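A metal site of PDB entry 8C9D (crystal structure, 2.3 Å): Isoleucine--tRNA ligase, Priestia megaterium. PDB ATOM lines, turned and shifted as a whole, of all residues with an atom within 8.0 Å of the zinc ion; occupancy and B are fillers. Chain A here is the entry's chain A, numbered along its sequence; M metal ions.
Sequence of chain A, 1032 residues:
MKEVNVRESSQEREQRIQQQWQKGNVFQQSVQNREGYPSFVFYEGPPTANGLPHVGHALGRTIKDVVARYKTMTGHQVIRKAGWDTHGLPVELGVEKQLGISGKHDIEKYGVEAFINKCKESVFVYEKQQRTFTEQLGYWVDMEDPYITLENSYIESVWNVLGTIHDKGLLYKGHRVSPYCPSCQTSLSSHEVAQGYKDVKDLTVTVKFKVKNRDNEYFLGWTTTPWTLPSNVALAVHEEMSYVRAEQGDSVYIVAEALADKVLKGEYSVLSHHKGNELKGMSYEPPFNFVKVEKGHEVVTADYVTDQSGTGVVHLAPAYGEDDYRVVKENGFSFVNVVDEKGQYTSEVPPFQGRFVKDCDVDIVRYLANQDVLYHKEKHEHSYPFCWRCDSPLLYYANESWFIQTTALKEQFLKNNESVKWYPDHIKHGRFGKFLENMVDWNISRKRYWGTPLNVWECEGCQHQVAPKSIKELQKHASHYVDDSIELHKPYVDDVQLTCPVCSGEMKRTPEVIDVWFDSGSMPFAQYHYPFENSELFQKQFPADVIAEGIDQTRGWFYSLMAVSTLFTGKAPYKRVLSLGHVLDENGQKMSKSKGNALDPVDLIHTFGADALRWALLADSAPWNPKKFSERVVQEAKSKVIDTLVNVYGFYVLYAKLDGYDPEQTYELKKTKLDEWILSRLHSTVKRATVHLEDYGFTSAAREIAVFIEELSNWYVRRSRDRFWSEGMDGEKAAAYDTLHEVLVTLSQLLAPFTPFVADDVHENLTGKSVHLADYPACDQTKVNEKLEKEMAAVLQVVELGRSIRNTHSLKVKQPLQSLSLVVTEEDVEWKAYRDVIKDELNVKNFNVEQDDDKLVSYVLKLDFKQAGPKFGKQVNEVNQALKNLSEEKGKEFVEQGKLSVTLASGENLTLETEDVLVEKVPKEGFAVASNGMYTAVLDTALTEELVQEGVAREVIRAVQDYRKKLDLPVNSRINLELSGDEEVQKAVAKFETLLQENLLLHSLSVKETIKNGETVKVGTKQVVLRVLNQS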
ATOM      1  N   GLU A 458     -24.535  -3.037   5.911  1.00  0.00           N
ATOM      2  CA  GLU A 458     -23.141  -3.452   5.990  1.00  0.00           C
ATOM      3  C   GLU A 458     -22.250  -2.326   5.505  1.00  0.00           C
ATOM      4  O   GLU A 458     -22.551  -1.667   4.513  1.00  0.00           O
ATOM      5  CB  GLU A 458     -22.879  -4.697   5.129  1.00  0.00           C
ATOM      6  CG  GLU A 458     -23.830  -5.865   5.360  1.00  0.00           C
ATOM      7  CD  GLU A 458     -23.580  -7.003   4.386  1.00  0.00           C
ATOM      8  OE1 GLU A 458     -24.441  -7.261   3.511  1.00  0.00           O
ATOM      9  OE2 GLU A 458     -22.509  -7.643   4.491  1.00  0.00           O
ATOM     10  N   CYS A 459     -21.152  -2.118   6.224  1.00  0.00           N
ATOM     11  CA  CYS A 459     -20.194  -1.087   5.869  1.00  0.00           C
ATOM     12  C   CYS A 459     -19.368  -1.522   4.660  1.00  0.00           C
ATOM     13  O   CYS A 459     -18.794  -2.621   4.655  1.00  0.00           O
ATOM     14  CB  CYS A 459     -19.278  -0.784   7.055  1.00  0.00           C
ATOM     15  SG  CYS A 459     -17.939   0.356   6.666  1.00  0.00           S
ATOM     16  N   GLU A 460     -19.318  -0.661   3.644  1.00  0.00           N
ATOM     17  CA  GLU A 460     -18.531  -0.967   2.441  1.00  0.00           C
ATOM     18  C   GLU A 460     -17.049  -1.101   2.757  1.00  0.00           C
ATOM     19  O   GLU A 460     -16.327  -1.811   2.062  1.00  0.00           O
ATOM     20  CB  GLU A 460     -18.746   0.125   1.388  1.00  0.00           C
ATOM     21  CG  GLU A 460     -20.187   0.299   0.954  1.00  0.00           C
ATOM     22  CD  GLU A 460     -20.626  -0.772  -0.024  1.00  0.00           C
ATOM     23  OE1 GLU A 460     -20.002  -0.885  -1.101  1.00  0.00           O
ATOM     24  OE2 GLU A 460     -21.597  -1.494   0.282  1.00  0.00           O
ATOM     25  N   GLY A 461     -16.588  -0.424   3.805  1.00  0.00           N
ATOM     26  CA  GLY A 461     -15.172  -0.412   4.136  1.00  0.00           C
ATOM     27  C   GLY A 461     -14.719  -1.593   4.965  1.00  0.00           C
ATOM     28  O   GLY A 461     -13.762  -2.278   4.596  1.00  0.00           O
ATOM     29  N   CYS A 462     -15.407  -1.857   6.080  1.00  0.00           N
ATOM     30  CA  CYS A 462     -14.978  -2.873   7.034  1.00  0.00           C
ATOM     31  C   CYS A 462     -16.000  -3.973   7.273  1.00  0.00           C
ATOM     32  O   CYS A 462     -15.755  -4.838   8.119  1.00  0.00           O
ATOM     33  CB  CYS A 462     -14.620  -2.229   8.375  1.00  0.00           C
ATOM     34  SG  CYS A 462     -16.047  -1.684   9.300  1.00  0.00           S
ATOM     35  N   GLN A 463     -17.150  -3.949   6.596  1.00  0.00           N
ATOM     36  CA  GLN A 463     -18.182  -4.992   6.603  1.00  0.00           C
ATOM     37  C   GLN A 463     -18.881  -5.150   7.939  1.00  0.00           C
ATOM     38  O   GLN A 463     -19.639  -6.117   8.128  1.00  0.00           O
ATOM     39  CB  GLN A 463     -17.613  -6.346   6.153  1.00  0.00           C
ATOM     40  CG  GLN A 463     -17.310  -6.414   4.665  1.00  0.00           C
ATOM     41  CD  GLN A 463     -16.126  -5.544   4.273  1.00  0.00           C
ATOM     42  OE1 GLN A 463     -15.031  -5.680   4.827  1.00  0.00           O
ATOM     43  NE2 GLN A 463     -16.349  -4.629   3.338  1.00  0.00           N
ATOM     44  N   HIS A 464     -18.668  -4.234   8.881  1.00  0.00           N
ATOM     45  CA  HIS A 464     -19.449  -4.203  10.113  1.00  0.00           C
ATOM     46  C   HIS A 464     -20.938  -4.141   9.777  1.00  0.00           C
ATOM     47  O   HIS A 464     -21.338  -3.549   8.766  1.00  0.00           O
ATOM     48  CB  HIS A 464     -19.023  -3.005  10.965  1.00  0.00           C
ATOM     49  CG  HIS A 464     -19.846  -2.809  12.203  1.00  0.00           C
ATOM     50  ND1 HIS A 464     -19.660  -3.552  13.354  1.00  0.00           N
ATOM     51  CD2 HIS A 464     -20.832  -1.921  12.486  1.00  0.00           C
ATOM     52  CE1 HIS A 464     -20.519  -3.147  14.272  1.00  0.00           C
ATOM     53  NE2 HIS A 464     -21.231  -2.160  13.772  1.00  0.00           N
ATOM     54  N   GLN A 465     -21.757  -4.772  10.615  1.00  0.00           N
ATOM     55  CA  GLN A 465     -23.192  -4.884  10.370  1.00  0.00           C
ATOM     56  C   GLN A 465     -23.977  -4.106  11.414  1.00  0.00           C
ATOM     57  O   GLN A 465     -23.648  -4.137  12.609  1.00  0.00           O
ATOM     58  CB  GLN A 465     -23.631  -6.345  10.379  1.00  0.00           C
ATOM     59  CG  GLN A 465     -23.012  -7.190   9.284  1.00  0.00           C
ATOM     60  CD  GLN A 465     -23.408  -8.649   9.362  1.00  0.00           C
ATOM     61  OE1 GLN A 465     -24.189  -9.046  10.227  1.00  0.00           O
ATOM     62  NE2 GLN A 465     -22.890  -9.462   8.449  1.00  0.00           N
ATOM     63  N   THR A 499     -23.844   5.706   8.674  1.00  0.00           N
ATOM     64  CA  THR A 499     -22.443   5.916   8.988  1.00  0.00           C
ATOM     65  C   THR A 499     -21.954   4.772   9.864  1.00  0.00           C
ATOM     66  O   THR A 499     -22.567   4.462  10.886  1.00  0.00           O
ATOM     67  CB  THR A 499     -22.218   7.255   9.681  1.00  0.00           C
ATOM     68  OG1 THR A 499     -22.991   8.271   9.034  1.00  0.00           O
ATOM     69  CG2 THR A 499     -20.749   7.637   9.623  1.00  0.00           C
ATOM     70  N   CYS A 500     -20.864   4.141   9.456  1.00  0.00           N
ATOM     71  CA  CYS A 500     -20.360   3.002  10.198  1.00  0.00           C
ATOM     72  C   CYS A 500     -19.829   3.455  11.564  1.00  0.00           C
ATOM     73  O   CYS A 500     -18.962   4.333  11.615  1.00  0.00           O
ATOM     74  CB  CYS A 500     -19.250   2.298   9.426  1.00  0.00           C
ATOM     75  SG  CYS A 500     -18.441   0.988  10.382  1.00  0.00           S
ATOM     76  N   PRO A 501     -20.302   2.875  12.669  1.00  0.00           N
ATOM     77  CA  PRO A 501     -19.769   3.268  13.980  1.00  0.00           C
ATOM     78  C   PRO A 501     -18.301   2.934  14.166  1.00  0.00           C
ATOM     79  O   PRO A 501     -17.680   3.483  15.087  1.00  0.00           O
ATOM     80  CB  PRO A 501     -20.645   2.479  14.966  1.00  0.00           C
ATOM     81  CG  PRO A 501     -21.226   1.354  14.156  1.00  0.00           C
ATOM     82  CD  PRO A 501     -21.407   1.912  12.778  1.00  0.00           C
ATOM     83  N   VAL A 502     -17.735   2.061  13.346  1.00  0.00           N
ATOM     84  CA  VAL A 502     -16.345   1.643  13.496  1.00  0.00           C
ATOM     85  C   VAL A 502     -15.413   2.549  12.698  1.00  0.00           C
ATOM     86  O   VAL A 502     -14.454   3.114  13.251  1.00  0.00           O
ATOM     87  CB  VAL A 502     -16.164   0.174  13.060  1.00  0.00           C
ATOM     88  CG1 VAL A 502     -14.686  -0.198  13.091  1.00  0.00           C
ATOM     89  CG2 VAL A 502     -16.969  -0.745  13.960  1.00  0.00           C
ATOM     90  N   CYS A 503     -15.649   2.688  11.392  1.00  0.00           N
ATOM     91  CA  CYS A 503     -14.728   3.412  10.528  1.00  0.00           C
ATOM     92  C   CYS A 503     -15.346   4.640   9.871  1.00  0.00           C
ATOM     93  O   CYS A 503     -14.660   5.294   9.071  1.00  0.00           O
ATOM     94  CB  CYS A 503     -14.164   2.480   9.457  1.00  0.00           C
ATOM     95  SG  CYS A 503     -15.333   2.053   8.150  1.00  0.00           S
ATOM     96  N   SER A 504     -16.604   4.974  10.168  1.00  0.00           N
ATOM     97  CA  SER A 504     -17.336   6.091   9.576  1.00  0.00           C
ATOM     98  C   SER A 504     -17.563   5.920   8.081  1.00  0.00           C
ATOM     99  O   SER A 504     -17.948   6.880   7.397  1.00  0.00           O
ATOM    100  CB  SER A 504     -16.633   7.431   9.857  1.00  0.00           C
ATOM    101  OG  SER A 504     -17.558   8.503   9.973  1.00  0.00           O
ATOM    102  N   GLY A 505     -17.345   4.718   7.539  1.00  0.00           N
ATOM    103  CA  GLY A 505     -17.596   4.469   6.133  1.00  0.00           C
ATOM    104  C   GLY A 505     -19.082   4.399   5.825  1.00  0.00           C
ATOM    105  O   GLY A 505     -19.949   4.566   6.688  1.00  0.00           O
ATOM    106  N   GLU A 506     -19.376   4.167   4.551  1.00  0.00           N
ATOM    107  CA  GLU A 506     -20.768   4.096   4.093  1.00  0.00           C
ATOM    108  C   GLU A 506     -21.338   2.714   4.350  1.00  0.00           C
ATOM    109  O   GLU A 506     -20.737   1.697   3.971  1.00  0.00           O
ATOM    110  CB  GLU A 506     -20.839   4.430   2.607  1.00  0.00           C
ATOM    111  CG  GLU A 506     -22.257   4.531   2.047  1.00  0.00           C
ATOM    112  CD  GLU A 506     -22.282   4.697   0.538  1.00  0.00           C
ATOM    113  OE1 GLU A 506     -21.327   4.255  -0.130  1.00  0.00           O
ATOM    114  OE2 GLU A 506     -23.257   5.276   0.014  1.00  0.00           O
ATOM    115  N   MET A 507     -22.502   2.661   5.001  1.00  0.00           N
ATOM    116  CA  MET A 507     -23.237   1.418   5.216  1.00  0.00           C
ATOM    117  C   MET A 507     -24.413   1.354   4.242  1.00  0.00           C
ATOM    118  O   MET A 507     -25.257   2.251   4.224  1.00  0.00           O
ATOM    119  CB  MET A 507     -23.740   1.315   6.658  1.00  0.00           C
ATOM    120  CG  MET A 507     -22.647   1.431   7.704  1.00  0.00           C
ATOM    121  SD  MET A 507     -23.251   0.911   9.326  1.00  0.00           S
ATOM    122  CE  MET A 507     -22.611  -0.760   9.409  1.00  0.00           C
HETATM  123 ZN    ZN M   1     -16.895   0.421   8.762  1.00  0.00          ZN
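N of Val 502 lies close to SG of Cys 500 (3.2 Å).
The backbone carbonyl oxygen (O) of Gly 505 is in hydrogen-bond range of the backbone NH (N) of Cys 500, at 2.9 Å.
The backbone NH of His 464 lies close to the side-chain sulfur of Cys 462.
SG of Cys 503 lies close to N of Gly 505, at 3.4 Å.
The backbone NH of Cys 459 is in hydrogen-bond range of the backbone carbonyl oxygen of His 464 (2.9 Å).
SG of Cys 459 lies close to N of Gly 461, at 3.3 Å.
NE2 of Gln 463 lies close to O of Cys 459, 3.4 Å away.
Within 4 Å of the zinc ion: Cys 459, Cys 462, Cys 500 and Cys 503.
The nearest printed residue that does not touch the zinc ion is Val 502 (4.4 Å).
The zinc ion is bound by SG of Cys 500, SG of Cys 462, SG of Cys 503 and SG of Cys 459.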
